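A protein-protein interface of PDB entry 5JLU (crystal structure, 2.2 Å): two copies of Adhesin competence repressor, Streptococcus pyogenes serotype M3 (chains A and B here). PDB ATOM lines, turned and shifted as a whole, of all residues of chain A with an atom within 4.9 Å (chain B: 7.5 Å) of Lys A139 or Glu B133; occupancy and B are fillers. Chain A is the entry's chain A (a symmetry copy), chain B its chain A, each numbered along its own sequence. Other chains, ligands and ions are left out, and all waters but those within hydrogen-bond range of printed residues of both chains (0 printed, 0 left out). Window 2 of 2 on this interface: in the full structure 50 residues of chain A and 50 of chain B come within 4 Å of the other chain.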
ATOM      1  N   GLU A 135      11.190  -2.942 -11.559  1.00  0.00           N
ATOM      2  CA  GLU A 135      12.660  -2.936 -11.864  1.00  0.00           C
ATOM      3  C   GLU A 135      13.472  -3.455 -10.665  1.00  0.00           C
ATOM      4  O   GLU A 135      14.497  -4.106 -10.812  1.00  0.00           O
ATOM      5  CB  GLU A 135      13.196  -1.532 -12.309  1.00  0.00           C
ATOM      6  CG  GLU A 135      12.470  -0.921 -13.530  1.00  0.00           C
ATOM      7  CD  GLU A 135      12.199  -1.944 -14.638  1.00  0.00           C
ATOM      8  OE1 GLU A 135      13.213  -2.423 -15.221  1.00  0.00           O
ATOM      9  OE2 GLU A 135      10.992  -2.293 -14.894  1.00  0.00           O
ATOM     10  N   ILE A 136      12.969  -3.170  -9.494  1.00  0.00           N
ATOM     11  CA  ILE A 136      13.606  -3.602  -8.281  1.00  0.00           C
ATOM     12  C   ILE A 136      13.318  -5.089  -8.071  1.00  0.00           C
ATOM     13  O   ILE A 136      14.201  -5.834  -7.691  1.00  0.00           O
ATOM     14  CB  ILE A 136      13.097  -2.807  -7.127  1.00  0.00           C
ATOM     15  CG1 ILE A 136      13.577  -1.351  -7.291  1.00  0.00           C
ATOM     16  CG2 ILE A 136      13.579  -3.372  -5.788  1.00  0.00           C
ATOM     17  CD1 ILE A 136      12.741  -0.427  -6.446  1.00  0.00           C
ATOM     18  N   VAL A 137      12.088  -5.511  -8.324  1.00  0.00           N
ATOM     19  CA  VAL A 137      11.782  -6.912  -8.236  1.00  0.00           C
ATOM     20  C   VAL A 137      12.684  -7.690  -9.194  1.00  0.00           C
ATOM     21  O   VAL A 137      13.252  -8.673  -8.792  1.00  0.00           O
ATOM     22  CB  VAL A 137      10.296  -7.189  -8.459  1.00  0.00           C
ATOM     23  CG1 VAL A 137      10.061  -8.686  -8.645  1.00  0.00           C
ATOM     24  CG2 VAL A 137       9.484  -6.627  -7.298  1.00  0.00           C
ATOM     25  N   ASP A 138      12.935  -7.152 -10.384  1.00  0.00           N
ATOM     26  CA  ASP A 138      13.800  -7.773 -11.355  1.00  0.00           C
ATOM     27  C   ASP A 138      15.174  -7.906 -10.819  1.00  0.00           C
ATOM     28  O   ASP A 138      15.767  -9.017 -10.808  1.00  0.00           O
ATOM     29  CB  ASP A 138      13.812  -6.945 -12.657  1.00  0.00           C
ATOM     30  CG  ASP A 138      14.640  -7.593 -13.809  1.00  0.00           C
ATOM     31  OD1 ASP A 138      15.226  -8.689 -13.663  1.00  0.00           O
ATOM     32  OD2 ASP A 138      14.705  -6.974 -14.891  1.00  0.00           O
ATOM     33  N   LYS A 139      15.697  -6.772 -10.379  1.00  0.00           N
ATOM     34  CA  LYS A 139      17.029  -6.721  -9.797  1.00  0.00           C
ATOM     35  C   LYS A 139      17.109  -7.761  -8.674  1.00  0.00           C
ATOM     36  O   LYS A 139      18.030  -8.530  -8.642  1.00  0.00           O
ATOM     37  CB  LYS A 139      17.377  -5.303  -9.317  1.00  0.00           C
ATOM     38  CG  LYS A 139      18.882  -5.003  -9.211  1.00  0.00           C
ATOM     39  CD  LYS A 139      19.215  -3.667  -8.497  1.00  0.00           C
ATOM     40  CE  LYS A 139      20.462  -3.782  -7.594  1.00  0.00           C
ATOM     41  NZ  LYS A 139      20.586  -2.635  -6.658  1.00  0.00           N
ATOM     42  N   PHE A 140      16.106  -7.850  -7.808  1.00  0.00           N
ATOM     43  CA  PHE A 140      16.143  -8.859  -6.744  1.00  0.00           C
ATOM     44  C   PHE A 140      16.147 -10.314  -7.274  1.00  0.00           C
ATOM     45  O   PHE A 140      17.027 -11.112  -6.899  1.00  0.00           O
ATOM     46  CB  PHE A 140      15.001  -8.633  -5.758  1.00  0.00           C
ATOM     47  CG  PHE A 140      14.847  -9.721  -4.781  1.00  0.00           C
ATOM     48  CD1 PHE A 140      15.813  -9.930  -3.817  1.00  0.00           C
ATOM     49  CD2 PHE A 140      13.740 -10.565  -4.839  1.00  0.00           C
ATOM     50  CE1 PHE A 140      15.679 -10.976  -2.926  1.00  0.00           C
ATOM     51  CE2 PHE A 140      13.613 -11.625  -3.971  1.00  0.00           C
ATOM     52  CZ  PHE A 140      14.585 -11.824  -3.017  1.00  0.00           C
ATOM     53  N   VAL A 141      15.234 -10.666  -8.172  1.00  0.00           N
ATOM     54  CA  VAL A 141      15.143 -12.072  -8.584  1.00  0.00           C
ATOM     55  C   VAL A 141      16.376 -12.477  -9.324  1.00  0.00           C
ATOM     56  O   VAL A 141      16.820 -13.631  -9.191  1.00  0.00           O
ATOM     57  CB  VAL A 141      13.863 -12.481  -9.367  1.00  0.00           C
ATOM     58  CG1 VAL A 141      12.631 -12.093  -8.601  1.00  0.00           C
ATOM     59  CG2 VAL A 141      13.803 -11.917 -10.753  1.00  0.00           C
ATOM     60  N   THR A 142      16.953 -11.519 -10.048  1.00  0.00           N
ATOM     61  CA  THR A 142      18.170 -11.749 -10.801  1.00  0.00           C
ATOM     62  C   THR A 142      19.328 -12.094  -9.882  1.00  0.00           C
ATOM     63  O   THR A 142      19.943 -13.148 -10.100  1.00  0.00           O
ATOM     64  CB  THR A 142      18.533 -10.559 -11.701  1.00  0.00           C
ATOM     65  OG1 THR A 142      17.456 -10.314 -12.605  1.00  0.00           O
ATOM     66  CG2 THR A 142      19.807 -10.861 -12.516  1.00  0.00           C
ATOM     67  N   VAL A 143      19.611 -11.253  -8.863  1.00  0.00           N
ATOM     68  CA  VAL A 143      20.731 -11.576  -7.960  1.00  0.00           C
ATOM     69  C   VAL A 143      20.498 -12.839  -7.106  1.00  0.00           C
ATOM     70  O   VAL A 143      21.418 -13.592  -6.798  1.00  0.00           O
ATOM     71  CB  VAL A 143      21.166 -10.399  -7.041  1.00  0.00           C
ATOM     72  CG1 VAL A 143      21.616  -9.204  -7.865  1.00  0.00           C
ATOM     73  CG2 VAL A 143      20.103  -9.964  -6.082  1.00  0.00           C
ATOM     74  N   LEU B   7       9.552 -11.189 -16.346  1.00  0.00           N
ATOM     75  CA  LEU B   7       9.786 -11.466 -14.937  1.00  0.00           C
ATOM     76  C   LEU B   7       9.086 -12.783 -14.492  1.00  0.00           C
ATOM     77  O   LEU B   7       9.589 -13.462 -13.634  1.00  0.00           O
ATOM     78  CB  LEU B   7       9.362 -10.326 -14.057  1.00  0.00           C
ATOM     79  CG  LEU B   7      10.432  -9.268 -13.782  1.00  0.00           C
ATOM     80  CD1 LEU B   7      11.421  -9.032 -14.921  1.00  0.00           C
ATOM     81  CD2 LEU B   7       9.763  -7.947 -13.383  1.00  0.00           C
ATOM     82  N   LYS B  10      11.461 -15.395 -15.169  1.00  0.00           N
ATOM     83  CA  LYS B  10      12.530 -15.478 -14.218  1.00  0.00           C
ATOM     84  C   LYS B  10      12.045 -16.052 -12.930  1.00  0.00           C
ATOM     85  O   LYS B  10      12.852 -16.687 -12.266  1.00  0.00           O
ATOM     86  CB  LYS B  10      13.152 -14.135 -13.900  1.00  0.00           C
ATOM     87  CG  LYS B  10      13.748 -13.455 -15.116  1.00  0.00           C
ATOM     88  CD  LYS B  10      14.454 -12.194 -14.649  1.00  0.00           C
ATOM     89  CE  LYS B  10      14.988 -11.422 -15.844  1.00  0.00           C
ATOM     90  NZ  LYS B  10      16.220 -10.697 -15.465  1.00  0.00           N
ATOM     91  N   LEU B 125      23.065 -10.680   0.197  1.00  0.00           N
ATOM     92  CA  LEU B 125      22.406 -10.299  -1.030  1.00  0.00           C
ATOM     93  C   LEU B 125      21.442  -9.113  -0.838  1.00  0.00           C
ATOM     94  O   LEU B 125      21.357  -8.217  -1.665  1.00  0.00           O
ATOM     95  CB  LEU B 125      21.745 -11.544  -1.489  1.00  0.00           C
ATOM     96  CG  LEU B 125      20.631 -11.852  -2.404  1.00  0.00           C
ATOM     97  CD1 LEU B 125      20.554 -13.400  -2.366  1.00  0.00           C
ATOM     98  CD2 LEU B 125      19.331 -11.234  -1.910  1.00  0.00           C
ATOM     99  N   LEU B 126      20.726  -9.118   0.287  1.00  0.00           N
ATOM    100  CA  LEU B 126      19.867  -8.066   0.622  1.00  0.00           C
ATOM    101  C   LEU B 126      20.658  -6.717   0.780  1.00  0.00           C
ATOM    102  O   LEU B 126      20.222  -5.661   0.291  1.00  0.00           O
ATOM    103  CB  LEU B 126      19.084  -8.485   1.864  1.00  0.00           C
ATOM    104  CG  LEU B 126      18.061  -9.604   1.595  1.00  0.00           C
ATOM    105  CD1 LEU B 126      17.455 -10.091   2.907  1.00  0.00           C
ATOM    106  CD2 LEU B 126      16.956  -9.193   0.669  1.00  0.00           C
ATOM    107  N   GLN B 127      21.863  -6.795   1.339  1.00  0.00           N
ATOM    108  CA  GLN B 127      22.727  -5.648   1.528  1.00  0.00           C
ATOM    109  C   GLN B 127      22.954  -4.825   0.288  1.00  0.00           C
ATOM    110  O   GLN B 127      23.234  -3.655   0.403  1.00  0.00           O
ATOM    111  CB  GLN B 127      24.093  -6.068   2.043  1.00  0.00           C
ATOM    112  CG  GLN B 127      24.097  -6.258   3.533  1.00  0.00           C
ATOM    113  CD  GLN B 127      25.497  -6.328   4.094  1.00  0.00           C
ATOM    114  OE1 GLN B 127      26.404  -5.676   3.585  1.00  0.00           O
ATOM    115  NE2 GLN B 127      25.663  -7.044   5.188  1.00  0.00           N
ATOM    116  N   LYS B 128      22.871  -5.433  -0.882  1.00  0.00           N
ATOM    117  CA  LYS B 128      22.968  -4.669  -2.152  1.00  0.00           C
ATOM    118  C   LYS B 128      21.823  -3.733  -2.502  1.00  0.00           C
ATOM    119  O   LYS B 128      21.869  -3.053  -3.531  1.00  0.00           O
ATOM    120  CB  LYS B 128      23.144  -5.655  -3.292  1.00  0.00           C
ATOM    121  CG  LYS B 128      24.418  -6.461  -3.140  1.00  0.00           C
ATOM    122  CD  LYS B 128      24.408  -7.715  -4.026  1.00  0.00           C
ATOM    123  CE  LYS B 128      25.829  -8.269  -4.144  1.00  0.00           C
ATOM    124  NZ  LYS B 128      25.944  -9.265  -5.233  1.00  0.00           N
ATOM    125  N   PHE B 129      20.794  -3.675  -1.670  1.00  0.00           N
ATOM    126  CA  PHE B 129      19.625  -2.868  -1.965  1.00  0.00           C
ATOM    127  C   PHE B 129      19.623  -1.774  -0.950  1.00  0.00           C
ATOM    128  O   PHE B 129      19.975  -2.024   0.209  1.00  0.00           O
ATOM    129  CB  PHE B 129      18.313  -3.727  -1.950  1.00  0.00           C
ATOM    130  CG  PHE B 129      18.280  -4.710  -3.094  1.00  0.00           C
ATOM    131  CD1 PHE B 129      18.888  -5.959  -2.975  1.00  0.00           C
ATOM    132  CD2 PHE B 129      17.803  -4.324  -4.321  1.00  0.00           C
ATOM    133  CE1 PHE B 129      18.916  -6.838  -4.060  1.00  0.00           C
ATOM    134  CE2 PHE B 129      17.805  -5.204  -5.406  1.00  0.00           C
ATOM    135  CZ  PHE B 129      18.379  -6.453  -5.283  1.00  0.00           C
ATOM    136  N   SER B 130      19.216  -0.575  -1.354  1.00  0.00           N
ATOM    137  CA  SER B 130      18.916   0.470  -0.335  1.00  0.00           C
ATOM    138  C   SER B 130      17.730   0.008   0.482  1.00  0.00           C
ATOM    139  O   SER B 130      17.012  -0.959   0.113  1.00  0.00           O
ATOM    140  CB  SER B 130      18.625   1.815  -0.984  1.00  0.00           C
ATOM    141  OG  SER B 130      17.420   1.761  -1.719  1.00  0.00           O
ATOM    142  N   ALA B 131      17.528   0.656   1.614  1.00  0.00           N
ATOM    143  CA  ALA B 131      16.390   0.330   2.488  1.00  0.00           C
ATOM    144  C   ALA B 131      15.006   0.679   1.891  1.00  0.00           C
ATOM    145  O   ALA B 131      13.991   0.080   2.267  1.00  0.00           O
ATOM    146  CB  ALA B 131      16.587   0.988   3.865  1.00  0.00           C
ATOM    147  N   LYS B 132      14.984   1.691   1.020  1.00  0.00           N
ATOM    148  CA  LYS B 132      13.881   1.941   0.092  1.00  0.00           C
ATOM    149  C   LYS B 132      13.591   0.731  -0.819  1.00  0.00           C
ATOM    150  O   LYS B 132      12.469   0.230  -0.868  1.00  0.00           O
ATOM    151  CB  LYS B 132      14.140   3.206  -0.782  1.00  0.00           C
ATOM    152  CG  LYS B 132      13.116   4.329  -0.598  1.00  0.00           C
ATOM    153  CD  LYS B 132      13.494   5.577  -1.416  1.00  0.00           C
ATOM    154  CE  LYS B 132      14.391   6.554  -0.641  1.00  0.00           C
ATOM    155  NZ  LYS B 132      14.430   7.892  -1.308  1.00  0.00           N
ATOM    156  N   GLU B 133      14.600   0.295  -1.541  1.00  0.00           N
ATOM    157  CA  GLU B 133      14.468  -0.903  -2.344  1.00  0.00           C
ATOM    158  C   GLU B 133      13.923  -2.081  -1.483  1.00  0.00           C
ATOM    159  O   GLU B 133      12.907  -2.682  -1.816  1.00  0.00           O
ATOM    160  CB  GLU B 133      15.796  -1.204  -3.064  1.00  0.00           C
ATOM    161  CG  GLU B 133      16.107  -0.179  -4.156  1.00  0.00           C
ATOM    162  CD  GLU B 133      17.525  -0.254  -4.715  1.00  0.00           C
ATOM    163  OE1 GLU B 133      18.469  -0.785  -4.034  1.00  0.00           O
ATOM    164  OE2 GLU B 133      17.696   0.215  -5.871  1.00  0.00           O
ATOM    165  N   LEU B 134      14.470  -2.294  -0.288  1.00  0.00           N
ATOM    166  CA  LEU B 134      14.059  -3.417   0.523  1.00  0.00           C
ATOM    167  C   LEU B 134      12.615  -3.386   0.965  1.00  0.00           C
ATOM    168  O   LEU B 134      12.088  -4.447   1.309  1.00  0.00           O
ATOM    169  CB  LEU B 134      15.003  -3.653   1.739  1.00  0.00           C
ATOM    170  CG  LEU B 134      16.402  -4.097   1.275  1.00  0.00           C
ATOM    171  CD1 LEU B 134      17.380  -4.097   2.430  1.00  0.00           C
ATOM    172  CD2 LEU B 134      16.417  -5.467   0.603  1.00  0.00           C
ATOM    173  N   GLU B 135      11.946  -2.231   1.008  1.00  0.00           N
ATOM    174  CA  GLU B 135      10.478  -2.272   1.315  1.00  0.00           C
ATOM    175  C   GLU B 135       9.698  -2.963   0.182  1.00  0.00           C
ATOM    176  O   GLU B 135       8.710  -3.649   0.403  1.00  0.00           O
ATOM    177  CB  GLU B 135       9.865  -0.860   1.605  1.00  0.00           C
ATOM    178  CG  GLU B 135      10.553  -0.080   2.750  1.00  0.00           C
ATOM    179  CD  GLU B 135      10.876  -0.959   3.962  1.00  0.00           C
ATOM    180  OE1 GLU B 135       9.888  -1.426   4.598  1.00  0.00           O
ATOM    181  OE2 GLU B 135      12.099  -1.212   4.251  1.00  0.00           O
ATOM    182  N   ILE B 136      10.189  -2.781  -1.015  1.00  0.00           N
ATOM    183  CA  ILE B 136       9.580  -3.376  -2.171  1.00  0.00           C
ATOM    184  C   ILE B 136       9.949  -4.860  -2.218  1.00  0.00           C
ATOM    185  O   ILE B 136       9.109  -5.689  -2.511  1.00  0.00           O
ATOM    186  CB  ILE B 136      10.048  -2.686  -3.406  1.00  0.00           C
ATOM    187  CG1 ILE B 136       9.490  -1.249  -3.401  1.00  0.00           C
ATOM    188  CG2 ILE B 136       9.602  -3.420  -4.674  1.00  0.00           C
ATOM    189  CD1 ILE B 136      10.277  -0.379  -4.345  1.00  0.00           C
ATOM    190  N   VAL B 137      11.200  -5.184  -1.924  1.00  0.00           N
ATOM    191  CA  VAL B 137      11.582  -6.568  -1.859  1.00  0.00           C
ATOM    192  C   VAL B 137      10.721  -7.284  -0.820  1.00  0.00           C
ATOM    193  O   VAL B 137      10.208  -8.335  -1.109  1.00  0.00           O
ATOM    194  CB  VAL B 137      13.080  -6.737  -1.612  1.00  0.00           C
ATOM    195  CG1 VAL B 137      13.395  -8.190  -1.264  1.00  0.00           C
ATOM    196  CG2 VAL B 137      13.863  -6.263  -2.830  1.00  0.00           C
ATOM    197  N   ASP B 138      10.436  -6.633   0.305  1.00  0.00           N
ATOM    198  CA  ASP B 138       9.604  -7.191   1.342  1.00  0.00           C
ATOM    199  C   ASP B 138       8.240  -7.457   0.827  1.00  0.00           C
ATOM    200  O   ASP B 138       7.710  -8.592   0.939  1.00  0.00           O
ATOM    201  CB  ASP B 138       9.543  -6.227   2.545  1.00  0.00           C
ATOM    202  CG  ASP B 138       8.748  -6.790   3.763  1.00  0.00           C
ATOM    203  OD1 ASP B 138       8.223  -7.926   3.740  1.00  0.00           O
ATOM    204  OD2 ASP B 138       8.646  -6.060   4.771  1.00  0.00           O
ATOM    205  N   LYS B 139       7.659  -6.407   0.267  1.00  0.00           N
ATOM    206  CA  LYS B 139       6.327  -6.493  -0.313  1.00  0.00           C
ATOM    207  C   LYS B 139       6.307  -7.652  -1.315  1.00  0.00           C
ATOM    208  O   LYS B 139       5.429  -8.469  -1.260  1.00  0.00           O
ATOM    209  CB  LYS B 139       5.904  -5.157  -0.944  1.00  0.00           C
ATOM    210  CG  LYS B 139       4.385  -4.952  -1.078  1.00  0.00           C
ATOM    211  CD  LYS B 139       3.982  -3.722  -1.932  1.00  0.00           C
ATOM    212  CE  LYS B 139       2.746  -4.004  -2.814  1.00  0.00           C
ATOM    213  NZ  LYS B 139       2.563  -2.974  -3.869  1.00  0.00           N
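Ile A136 touches its own counterpart, Ile B136. 5 positions are printed for both chains.
The side-chain amino group of Lys B10 is in hydrogen-bond range of the side-chain hydroxyl of Thr A142 (3.1 Å). NZ of Lys B10 is in salt-bridge range of OD1 of Asp A138 (2.9 Å). The backbone carbonyl oxygen of Lys B128 is in hydrogen-bond range of the side-chain amino group of Lys A139 (3.4 Å). OE1 of Glu B133 is in salt-bridge range of NZ of Lys A139, 3.8 Å away.
Of chain B, only Lys B128 (3.4 Å), Phe B129 (3.7 Å) and Glu B133 (3.8 Å) come within 4 Å of Lys A139. Of the printed residues of chain B, Val A143 touches Phe B129. Of the printed residues of chain A, Leu B125 touches Phe A140. Printed residues of chain A within 4 Å of Val B137: Phe A140. Printed residues of chain B within 4 Å of Asp A138: Leu B7 and Lys B10. The nearest residue of chain B that does not touch Lys A139 is Ser B130 (5.9 Å).
Printed residues of chain B that touch a printed residue of chain A: Leu B7, Lys B10, Leu B125, Lys B128, Phe B129, Glu B133, Ile B136 and Val B137. Hydrophobic or aromatic side chains of chain B that line the printed part of chain A: Leu B7, Leu B125, Phe B129, Ile B136 and Val B137. Among the printed residues, 12 pairs touch across the chains. Among the printed residues, Asp or Glu carboxylates within 4 Å of a Lys or Arg side-chain nitrogen of the other chain: Asp A138 with Lys B10 and Lys A139 with Glu B133.
The backbone carbonyl oxygen of Asp A138 sits at hydrogen-bond distance from the side-chain hydroxyl of Thr A142, 2.8 Å away. OE1 of Glu B133 sits at hydrogen-bond distance from N of Ser B130 (2.8 Å).
CD1 of Ile A136 touches CD1 of Ile B136 (3.2 Å). Asp A138 touches Leu B7 (CG to CD1, 3.7 Å). CE of Lys A139 touches CE2 of Phe B129, at 3.7 Å. Leu B125 touches Phe A140 (CD2 to CE1, 3.8 Å). Phe A140 touches Phe B129 (CA to CZ, 3.6 Å). Phe A140 touches Val B137 (CD1 to CG1, 3.9 Å). CG2 of Val A141 touches CB of Lys B10 (3.9 Å). Phe B129 touches Val A143.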
